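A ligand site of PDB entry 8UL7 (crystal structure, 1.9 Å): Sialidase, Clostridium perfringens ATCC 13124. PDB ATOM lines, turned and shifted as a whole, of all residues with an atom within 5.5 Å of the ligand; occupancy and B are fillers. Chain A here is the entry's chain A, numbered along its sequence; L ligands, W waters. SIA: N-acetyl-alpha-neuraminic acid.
Water W2 lies within hydrogen-bond range of an oxygen (O10) of the ligand, the backbone NH (N) of Trp 125 and a ring nitrogen (NE2) of His 64.
Water W1 lies within hydrogen-bond range of OD2 of Asp 248, OG of Ser 230, O8 of the ligand and NE of Arg 246.
Water W7 lies within hydrogen-bond range of the side-chain amide oxygen of Gln 193 (2.5 Å), an oxygen (O8) of the ligand (2.9 Å) and the indole nitrogen of Trp 125 (3.0 Å).
Water W5 lies within hydrogen-bond range of a ring nitrogen (NE2) of His 64, an oxygen (O7) of the ligand, the side-chain carboxylate of Asp 63 and the side-chain amide nitrogen of Asn 124.
Water W4 lies within hydrogen-bond range of NH2 of Arg 246 (3.0 Å), O1A of the ligand (3.2 Å) and OH of Tyr 311 (3.2 Å).
Merely in contact with the ligand: Ile 39 (3.5 Å), Met 100 (3.8 Å), Trp 119 (3.9 Å) and Glu 231 (3.7 Å).
Hydrophobic or aromatic side chains that line the ligand: Ile 39, Met 100, Trp 119, Trp 125 and Tyr 348.
Within 4 Å of the ligand: Arg 38, Ile 39, Arg 57, Asp 63, Met 100, Asp 101, Trp 119, Asn 124, Trp 125, Glu 231, Arg 246, Arg 313 and Tyr 348.
An oxygen (O2) of the ligand is in hydrogen-bond range of the side-chain carboxylate of Asp 63, at 2.7 Å.
The side-chain carboxylate (OD2) of Asp 101 sits at hydrogen-bond distance from a nitrogen (N5) of the ligand.
NH1 of Arg 38 is in salt-bridge range of O1B of the ligand (2.8 Å).
The guanidinium group of Arg 313 lies within salt-bridge range of an oxygen (O1B) of the ligand (2.9 Å).
O4 of the ligand lies within hydrogen-bond range of NH2 of Arg 57 (3.0 Å).
The guanidinium group (NH1) of Arg 246 is in salt-bridge range of an oxygen (O1A) of the ligand (3.0 Å).
OH of Tyr 348 sits close to O6 of the ligand (3.0 Å).
ND2 of Asn 124 sits at hydrogen-bond distance from O9 of the ligand (3.1 Å).
NE1 of Trp 125 sits at hydrogen-bond distance from O9 of the ligand.
The backbone NH (N) of Asp 101 lies within hydrogen-bond range of the side-chain carboxylate (OD1) of Asp 55 (3.2 Å).
The backbone carbonyl oxygen (O) of Arg 38 sits at hydrogen-bond distance from the backbone NH (N) of Asp 55.
NH2 of Arg 313 is in hydrogen-bond range of O of Gly 282 (2.9 Å).
OD2 of Asp 55 lies within salt-bridge range of NH2 of Arg 57, at 3.0 Å.
The guanidinium group (NH1) of Arg 246 lies within hydrogen-bond range of the side-chain hydroxyl (OH) of Tyr 348 (2.9 Å).
The guanidinium group (NH2) of Arg 246 sits at hydrogen-bond distance from the backbone carbonyl oxygen (O) of Gly 282, at 3.3 Å.
The side-chain hydroxyl of Tyr 348 lies within hydrogen-bond range of the side-chain carboxylate of Glu 231, 2.5 Å away.
The side-chain amide oxygen (OD1) of Asn 124 lies within hydrogen-bond range of the backbone NH (N) of Ala 126.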
ATOM      1  N   ARG A  38     -29.820   9.959  -1.775  1.00  0.00           N
ATOM      2  CA  ARG A  38     -28.695  10.902  -1.924  1.00  0.00           C
ATOM      3  C   ARG A  38     -29.094  12.022  -2.858  1.00  0.00           C
ATOM      4  O   ARG A  38     -30.025  11.892  -3.667  1.00  0.00           O
ATOM      5  CB  ARG A  38     -27.434  10.210  -2.472  1.00  0.00           C
ATOM      6  CG  ARG A  38     -26.649   9.395  -1.446  1.00  0.00           C
ATOM      7  CD  ARG A  38     -25.135   9.469  -1.732  1.00  0.00           C
ATOM      8  NE  ARG A  38     -24.598  10.793  -1.411  1.00  0.00           N
ATOM      9  CZ  ARG A  38     -23.383  11.199  -1.734  1.00  0.00           C
ATOM     10  NH1 ARG A  38     -22.514  10.395  -2.302  1.00  0.00           N
ATOM     11  NH2 ARG A  38     -23.053  12.473  -1.528  1.00  0.00           N
ATOM     12  N   ILE A  39     -28.341  13.126  -2.781  1.00  0.00           N
ATOM     13  CA  ILE A  39     -28.402  14.235  -3.744  1.00  0.00           C
ATOM     14  C   ILE A  39     -29.740  14.971  -3.716  1.00  0.00           C
ATOM     15  O   ILE A  39     -30.477  14.975  -4.713  1.00  0.00           O
ATOM     16  CB  ILE A  39     -28.121  13.752  -5.179  1.00  0.00           C
ATOM     17  CG1 ILE A  39     -27.079  12.624  -5.227  1.00  0.00           C
ATOM     18  CG2 ILE A  39     -27.710  14.956  -6.060  1.00  0.00           C
ATOM     19  CD1 ILE A  39     -25.708  12.948  -4.672  1.00  0.00           C
ATOM     20  N   ASP A  55     -32.183  11.409  -5.394  1.00  0.00           N
ATOM     21  CA  ASP A  55     -31.875  10.085  -5.916  1.00  0.00           C
ATOM     22  C   ASP A  55     -32.552   9.026  -5.055  1.00  0.00           C
ATOM     23  O   ASP A  55     -32.427   9.057  -3.832  1.00  0.00           O
ATOM     24  CB  ASP A  55     -30.368   9.793  -5.883  1.00  0.00           C
ATOM     25  CG  ASP A  55     -29.555  10.517  -6.967  1.00  0.00           C
ATOM     26  OD1 ASP A  55     -30.047  11.444  -7.667  1.00  0.00           O
ATOM     27  OD2 ASP A  55     -28.392  10.090  -7.099  1.00  0.00           O
ATOM     28  N   ARG A  57     -31.633   5.612  -4.320  1.00  0.00           N
ATOM     29  CA  ARG A  57     -30.529   4.665  -4.471  1.00  0.00           C
ATOM     30  C   ARG A  57     -30.960   3.325  -3.873  1.00  0.00           C
ATOM     31  O   ARG A  57     -30.623   2.947  -2.750  1.00  0.00           O
ATOM     32  CB  ARG A  57     -29.275   5.230  -3.835  1.00  0.00           C
ATOM     33  CG  ARG A  57     -28.939   6.664  -4.302  1.00  0.00           C
ATOM     34  CD  ARG A  57     -27.462   6.786  -4.610  1.00  0.00           C
ATOM     35  NE  ARG A  57     -27.114   8.024  -5.305  1.00  0.00           N
ATOM     36  CZ  ARG A  57     -25.869   8.451  -5.440  1.00  0.00           C
ATOM     37  NH1 ARG A  57     -24.852   7.774  -4.936  1.00  0.00           N
ATOM     38  NH2 ARG A  57     -25.635   9.576  -6.133  1.00  0.00           N
ATOM     39  N   ASP A  63     -22.770   5.252  -6.141  1.00  0.00           N
ATOM     40  CA  ASP A  63     -23.071   6.070  -7.310  1.00  0.00           C
ATOM     41  C   ASP A  63     -23.355   5.224  -8.546  1.00  0.00           C
ATOM     42  O   ASP A  63     -24.170   5.605  -9.395  1.00  0.00           O
ATOM     43  CB  ASP A  63     -21.893   6.974  -7.717  1.00  0.00           C
ATOM     44  CG  ASP A  63     -21.468   7.970  -6.655  1.00  0.00           C
ATOM     45  OD1 ASP A  63     -22.279   8.323  -5.764  1.00  0.00           O
ATOM     46  OD2 ASP A  63     -20.309   8.460  -6.789  1.00  0.00           O
ATOM     47  N   HIS A  64     -22.601   4.137  -8.716  1.00  0.00           N
ATOM     48  CA  HIS A  64     -22.653   3.325  -9.928  1.00  0.00           C
ATOM     49  C   HIS A  64     -23.554   2.132  -9.645  1.00  0.00           C
ATOM     50  O   HIS A  64     -23.106   1.063  -9.241  1.00  0.00           O
ATOM     51  CB  HIS A  64     -21.265   2.920 -10.352  1.00  0.00           C
ATOM     52  CG  HIS A  64     -20.334   4.082 -10.465  1.00  0.00           C
ATOM     53  ND1 HIS A  64     -19.008   4.006 -10.096  1.00  0.00           N
ATOM     54  CD2 HIS A  64     -20.538   5.352 -10.873  1.00  0.00           C
ATOM     55  CE1 HIS A  64     -18.439   5.187 -10.269  1.00  0.00           C
ATOM     56  NE2 HIS A  64     -19.346   6.016 -10.757  1.00  0.00           N
ATOM     57  N   MET A 100     -29.638  10.565 -12.215  1.00  0.00           N
ATOM     58  CA  MET A 100     -29.141  11.002 -10.905  1.00  0.00           C
ATOM     59  C   MET A 100     -28.640  12.446 -10.993  1.00  0.00           C
ATOM     60  O   MET A 100     -28.541  13.035 -12.080  1.00  0.00           O
ATOM     61  CB  MET A 100     -28.045  10.043 -10.450  1.00  0.00           C
ATOM     62  CG  MET A 100     -26.791  10.105 -11.348  1.00  0.00           C
ATOM     63  SD  MET A 100     -25.673   8.704 -11.102  1.00  0.00           S
ATOM     64  CE  MET A 100     -25.181   8.958  -9.395  1.00  0.00           C
ATOM     65  N   ASP A 101     -28.357  13.013  -9.825  1.00  0.00           N
ATOM     66  CA  ASP A 101     -27.654  14.287  -9.671  1.00  0.00           C
ATOM     67  C   ASP A 101     -28.480  15.431 -10.220  1.00  0.00           C
ATOM     68  O   ASP A 101     -28.030  16.152 -11.125  1.00  0.00           O
ATOM     69  CB  ASP A 101     -26.289  14.250 -10.356  1.00  0.00           C
ATOM     70  CG  ASP A 101     -25.224  13.544  -9.526  1.00  0.00           C
ATOM     71  OD1 ASP A 101     -25.542  12.917  -8.502  1.00  0.00           O
ATOM     72  OD2 ASP A 101     -24.035  13.633  -9.910  1.00  0.00           O
ATOM     73  N   TRP A 119     -26.739   7.192 -17.122  1.00  0.00           N
ATOM     74  CA  TRP A 119     -25.785   6.186 -17.555  1.00  0.00           C
ATOM     75  C   TRP A 119     -26.415   4.817 -17.357  1.00  0.00           C
ATOM     76  O   TRP A 119     -27.488   4.701 -16.763  1.00  0.00           O
ATOM     77  CB  TRP A 119     -24.462   6.273 -16.779  1.00  0.00           C
ATOM     78  CG  TRP A 119     -23.755   7.575 -16.942  1.00  0.00           C
ATOM     79  CD1 TRP A 119     -22.795   7.887 -17.867  1.00  0.00           C
ATOM     80  CD2 TRP A 119     -23.983   8.765 -16.186  1.00  0.00           C
ATOM     81  NE1 TRP A 119     -22.415   9.206 -17.721  1.00  0.00           N
ATOM     82  CE2 TRP A 119     -23.119   9.762 -16.697  1.00  0.00           C
ATOM     83  CE3 TRP A 119     -24.829   9.076 -15.120  1.00  0.00           C
ATOM     84  CZ2 TRP A 119     -23.067  11.060 -16.170  1.00  0.00           C
ATOM     85  CZ3 TRP A 119     -24.777  10.382 -14.580  1.00  0.00           C
ATOM     86  CH2 TRP A 119     -23.900  11.345 -15.113  1.00  0.00           C
ATOM     87  N   ASN A 124     -16.877   5.761 -13.102  1.00  0.00           N
ATOM     88  CA  ASN A 124     -17.094   7.190 -12.935  1.00  0.00           C
ATOM     89  C   ASN A 124     -17.348   7.868 -14.275  1.00  0.00           C
ATOM     90  O   ASN A 124     -16.662   7.605 -15.265  1.00  0.00           O
ATOM     91  CB  ASN A 124     -15.866   7.822 -12.257  1.00  0.00           C
ATOM     92  CG  ASN A 124     -15.984   9.332 -12.155  1.00  0.00           C
ATOM     93  OD1 ASN A 124     -15.509  10.068 -13.036  1.00  0.00           O
ATOM     94  ND2 ASN A 124     -16.659   9.799 -11.100  1.00  0.00           N
ATOM     95  N   TRP A 125     -18.344   8.761 -14.288  1.00  0.00           N
ATOM     96  CA  TRP A 125     -18.766   9.423 -15.513  1.00  0.00           C
ATOM     97  C   TRP A 125     -17.645  10.196 -16.198  1.00  0.00           C
ATOM     98  O   TRP A 125     -17.623  10.299 -17.434  1.00  0.00           O
ATOM     99  CB  TRP A 125     -19.926  10.387 -15.216  1.00  0.00           C
ATOM    100  CG  TRP A 125     -19.550  11.663 -14.502  1.00  0.00           C
ATOM    101  CD1 TRP A 125     -19.501  11.864 -13.137  1.00  0.00           C
ATOM    102  CD2 TRP A 125     -19.196  12.929 -15.098  1.00  0.00           C
ATOM    103  NE1 TRP A 125     -19.152  13.170 -12.858  1.00  0.00           N
ATOM    104  CE2 TRP A 125     -18.954  13.840 -14.044  1.00  0.00           C
ATOM    105  CE3 TRP A 125     -19.036  13.382 -16.416  1.00  0.00           C
ATOM    106  CZ2 TRP A 125     -18.581  15.174 -14.266  1.00  0.00           C
ATOM    107  CZ3 TRP A 125     -18.687  14.717 -16.638  1.00  0.00           C
ATOM    108  CH2 TRP A 125     -18.458  15.594 -15.572  1.00  0.00           C
ATOM    109  N   ALA A 126     -16.727  10.773 -15.425  1.00  0.00           N
ATOM    110  CA  ALA A 126     -15.776  11.707 -16.004  1.00  0.00           C
ATOM    111  C   ALA A 126     -14.468  11.046 -16.437  1.00  0.00           C
ATOM    112  O   ALA A 126     -13.804  11.541 -17.365  1.00  0.00           O
ATOM    113  CB  ALA A 126     -15.465  12.848 -15.016  1.00  0.00           C
ATOM    114  N   LEU A 174     -23.107  17.067 -17.207  1.00  0.00           N
ATOM    115  CA  LEU A 174     -24.407  17.041 -16.547  1.00  0.00           C
ATOM    116  C   LEU A 174     -24.550  18.367 -15.799  1.00  0.00           C
ATOM    117  O   LEU A 174     -23.671  19.220 -15.864  1.00  0.00           O
ATOM    118  CB  LEU A 174     -24.521  15.814 -15.622  1.00  0.00           C
ATOM    119  CG  LEU A 174     -23.562  15.775 -14.441  1.00  0.00           C
ATOM    120  CD1 LEU A 174     -24.275  15.228 -13.224  1.00  0.00           C
ATOM    121  CD2 LEU A 174     -22.308  14.989 -14.790  1.00  0.00           C
ATOM    122  N   GLN A 193     -21.260  20.821 -15.400  1.00  0.00           N
ATOM    123  CA  GLN A 193     -19.934  20.281 -15.167  1.00  0.00           C
ATOM    124  C   GLN A 193     -19.627  19.362 -16.339  1.00  0.00           C
ATOM    125  O   GLN A 193     -20.495  18.594 -16.752  1.00  0.00           O
ATOM    126  CB  GLN A 193     -19.872  19.512 -13.832  1.00  0.00           C
ATOM    127  CG  GLN A 193     -20.935  18.359 -13.693  1.00  0.00           C
ATOM    128  CD  GLN A 193     -20.845  17.648 -12.319  1.00  0.00           C
ATOM    129  OE1 GLN A 193     -19.748  17.286 -11.876  1.00  0.00           O
ATOM    130  NE2 GLN A 193     -21.988  17.427 -11.686  1.00  0.00           N
ATOM    131  N   SER A 230     -16.209  21.121 -10.431  1.00  0.00           N
ATOM    132  CA  SER A 230     -17.305  20.265 -10.877  1.00  0.00           C
ATOM    133  C   SER A 230     -18.641  20.824 -10.423  1.00  0.00           C
ATOM    134  O   SER A 230     -19.075  21.852 -10.959  1.00  0.00           O
ATOM    135  CB  SER A 230     -17.118  18.816 -10.375  1.00  0.00           C
ATOM    136  OG  SER A 230     -17.057  18.770  -8.947  1.00  0.00           O
ATOM    137  N   GLU A 231     -19.257  20.182  -9.436  1.00  0.00           N
ATOM    138  CA  GLU A 231     -20.572  20.639  -8.960  1.00  0.00           C
ATOM    139  C   GLU A 231     -20.524  22.100  -8.542  1.00  0.00           C
ATOM    140  O   GLU A 231     -19.601  22.535  -7.855  1.00  0.00           O
ATOM    141  CB  GLU A 231     -21.019  19.777  -7.768  1.00  0.00           C
ATOM    142  CG  GLU A 231     -21.255  18.305  -8.182  1.00  0.00           C
ATOM    143  CD  GLU A 231     -20.920  17.352  -7.078  1.00  0.00           C
ATOM    144  OE1 GLU A 231     -20.180  17.730  -6.143  1.00  0.00           O
ATOM    145  OE2 GLU A 231     -21.384  16.191  -7.123  1.00  0.00           O
ATOM    146  N   ARG A 246     -17.275  23.462  -6.343  1.00  0.00           N
ATOM    147  CA  ARG A 246     -16.475  22.414  -5.738  1.00  0.00           C
ATOM    148  C   ARG A 246     -15.137  22.311  -6.475  1.00  0.00           C
ATOM    149  O   ARG A 246     -15.114  22.053  -7.670  1.00  0.00           O
ATOM    150  CB  ARG A 246     -17.231  21.090  -5.820  1.00  0.00           C
ATOM    151  CG  ARG A 246     -16.399  19.855  -5.406  1.00  0.00           C
ATOM    152  CD  ARG A 246     -17.245  18.586  -5.475  1.00  0.00           C
ATOM    153  NE  ARG A 246     -16.460  17.380  -5.180  1.00  0.00           N
ATOM    154  CZ  ARG A 246     -17.022  16.205  -4.910  1.00  0.00           C
ATOM    155  NH1 ARG A 246     -18.333  16.063  -4.853  1.00  0.00           N
ATOM    156  NH2 ARG A 246     -16.237  15.139  -4.685  1.00  0.00           N
ATOM    157  N   ASP A 248     -11.796  20.325  -6.226  1.00  0.00           N
ATOM    158  CA  ASP A 248     -11.327  19.139  -5.516  1.00  0.00           C
ATOM    159  C   ASP A 248      -9.846  19.209  -5.151  1.00  0.00           C
ATOM    160  O   ASP A 248      -9.006  19.497  -6.006  1.00  0.00           O
ATOM    161  CB  ASP A 248     -11.587  17.895  -6.363  1.00  0.00           C
ATOM    162  CG  ASP A 248     -13.059  17.491  -6.346  1.00  0.00           C
ATOM    163  OD1 ASP A 248     -13.729  17.742  -5.299  1.00  0.00           O
ATOM    164  OD2 ASP A 248     -13.540  16.910  -7.342  1.00  0.00           O
ATOM    165  N   GLY A 282     -13.410  17.643  -2.486  1.00  0.00           N
ATOM    166  CA  GLY A 282     -14.402  18.661  -2.211  1.00  0.00           C
ATOM    167  C   GLY A 282     -15.763  18.025  -1.965  1.00  0.00           C
ATOM    168  O   GLY A 282     -15.902  16.813  -1.806  1.00  0.00           O
ATOM    169  N   TYR A 311     -14.173  12.204   3.418  1.00  0.00           N
ATOM    170  CA  TYR A 311     -15.593  12.028   3.145  1.00  0.00           C
ATOM    171  C   TYR A 311     -16.453  12.085   4.393  1.00  0.00           C
ATOM    172  O   TYR A 311     -17.667  11.863   4.310  1.00  0.00           O
ATOM    173  CB  TYR A 311     -15.830  10.718   2.389  1.00  0.00           C
ATOM    174  CG  TYR A 311     -15.247  10.809   0.995  1.00  0.00           C
ATOM    175  CD1 TYR A 311     -15.824  11.606   0.041  1.00  0.00           C
ATOM    176  CD2 TYR A 311     -14.083  10.117   0.654  1.00  0.00           C
ATOM    177  CE1 TYR A 311     -15.308  11.710  -1.245  1.00  0.00           C
ATOM    178  CE2 TYR A 311     -13.546  10.214  -0.654  1.00  0.00           C
ATOM    179  CZ  TYR A 311     -14.185  11.022  -1.590  1.00  0.00           C
ATOM    180  OH  TYR A 311     -13.706  11.181  -2.887  1.00  0.00           O
ATOM    181  N   ARG A 313     -17.224  14.846   6.046  1.00  0.00           N
ATOM    182  CA  ARG A 313     -18.101  15.946   5.657  1.00  0.00           C
ATOM    183  C   ARG A 313     -19.014  16.351   6.830  1.00  0.00           C
ATOM    184  O   ARG A 313     -20.233  16.536   6.669  1.00  0.00           O
ATOM    185  CB  ARG A 313     -18.910  15.543   4.420  1.00  0.00           C
ATOM    186  CG  ARG A 313     -18.067  15.594   3.138  1.00  0.00           C
ATOM    187  CD  ARG A 313     -18.648  14.711   2.037  1.00  0.00           C
ATOM    188  NE  ARG A 313     -17.899  14.841   0.796  1.00  0.00           N
ATOM    189  CZ  ARG A 313     -18.297  14.302  -0.341  1.00  0.00           C
ATOM    190  NH1 ARG A 313     -19.407  13.554  -0.404  1.00  0.00           N
ATOM    191  NH2 ARG A 313     -17.592  14.519  -1.454  1.00  0.00           N
ATOM    192  N   GLY A 345     -21.559   8.132   1.846  1.00  0.00           N
ATOM    193  CA  GLY A 345     -22.175   9.096   0.964  1.00  0.00           C
ATOM    194  C   GLY A 345     -23.028  10.065   1.754  1.00  0.00           C
ATOM    195  O   GLY A 345     -24.099   9.690   2.226  1.00  0.00           O
ATOM    196  N   GLY A 346     -22.559  11.298   1.938  1.00  0.00           N
ATOM    197  CA  GLY A 346     -23.265  12.290   2.734  1.00  0.00           C
ATOM    198  C   GLY A 346     -22.731  13.665   2.382  1.00  0.00           C
ATOM    199  O   GLY A 346     -21.882  13.818   1.494  1.00  0.00           O
ATOM    200  N   TYR A 348     -24.227  16.453   1.060  1.00  0.00           N
ATOM    201  CA  TYR A 348     -24.779  17.324   0.028  1.00  0.00           C
ATOM    202  C   TYR A 348     -25.971  18.099   0.601  1.00  0.00           C
ATOM    203  O   TYR A 348     -26.575  17.682   1.589  1.00  0.00           O
ATOM    204  CB  TYR A 348     -25.210  16.529  -1.225  1.00  0.00           C
ATOM    205  CG  TYR A 348     -24.096  16.116  -2.190  1.00  0.00           C
ATOM    206  CD1 TYR A 348     -22.807  15.823  -1.744  1.00  0.00           C
ATOM    207  CD2 TYR A 348     -24.342  16.040  -3.553  1.00  0.00           C
ATOM    208  CE1 TYR A 348     -21.784  15.444  -2.632  1.00  0.00           C
ATOM    209  CE2 TYR A 348     -23.343  15.639  -4.444  1.00  0.00           C
ATOM    210  CZ  TYR A 348     -22.062  15.385  -3.990  1.00  0.00           C
ATOM    211  OH  TYR A 348     -21.084  15.028  -4.899  1.00  0.00           O
HETATM  212  C1  SIA L   1     -19.753  12.547  -3.829  1.00  0.00           C
HETATM  213  C2  SIA L   1     -20.314  11.915  -5.203  1.00  0.00           C
HETATM  214  C3  SIA L   1     -21.863  11.924  -5.385  1.00  0.00           C
HETATM  215  C4  SIA L   1     -22.441  12.264  -6.771  1.00  0.00           C
HETATM  216  C5  SIA L   1     -21.403  11.896  -7.839  1.00  0.00           C
HETATM  217  C6  SIA L   1     -20.148  12.792  -7.633  1.00  0.00           C
HETATM  218  C7  SIA L   1     -18.909  12.343  -8.481  1.00  0.00           C
HETATM  219  C8  SIA L   1     -17.623  13.164  -8.144  1.00  0.00           C
HETATM  220  C9  SIA L   1     -16.453  12.720  -9.038  1.00  0.00           C
HETATM  221  C10 SIA L   1     -21.659  11.165 -10.236  1.00  0.00           C
HETATM  222  C11 SIA L   1     -22.433  11.430 -11.546  1.00  0.00           C
HETATM  223  N5  SIA L   1     -22.000  11.983  -9.193  1.00  0.00           N
HETATM  224  O1A SIA L   1     -18.714  13.278  -3.891  1.00  0.00           O
HETATM  225  O1B SIA L   1     -20.404  12.239  -2.785  1.00  0.00           O
HETATM  226  O2  SIA L   1     -19.813  10.601  -5.303  1.00  0.00           O
HETATM  227  O4  SIA L   1     -23.641  11.528  -7.101  1.00  0.00           O
HETATM  228  O6  SIA L   1     -19.669  12.718  -6.281  1.00  0.00           O
HETATM  229  O7  SIA L   1     -18.692  10.936  -8.404  1.00  0.00           O
HETATM  230  O8  SIA L   1     -17.922  14.565  -8.252  1.00  0.00           O
HETATM  231  O9  SIA L   1     -16.780  12.815 -10.443  1.00  0.00           O
HETATM  232  O10 SIA L   1     -20.786  10.287 -10.168  1.00  0.00           O
HETATM  233  O   HOH W   1     -15.927  16.392  -8.435  1.00  0.00           O
HETATM  234  O   HOH W   2     -20.067   8.626 -11.955  1.00  0.00           O
HETATM  235  O   HOH W   3     -16.976  10.112  -6.532  1.00  0.00           O
HETATM  236  O   HOH W   4     -15.929  12.134  -5.005  1.00  0.00           O
HETATM  237  O   HOH W   5     -18.246   8.074  -8.985  1.00  0.00           O
HETATM  238  O   HOH W   6     -16.006  14.997 -11.258  1.00  0.00           O
HETATM  239  O   HOH W   7     -19.437  15.101 -10.632  1.00  0.00           O
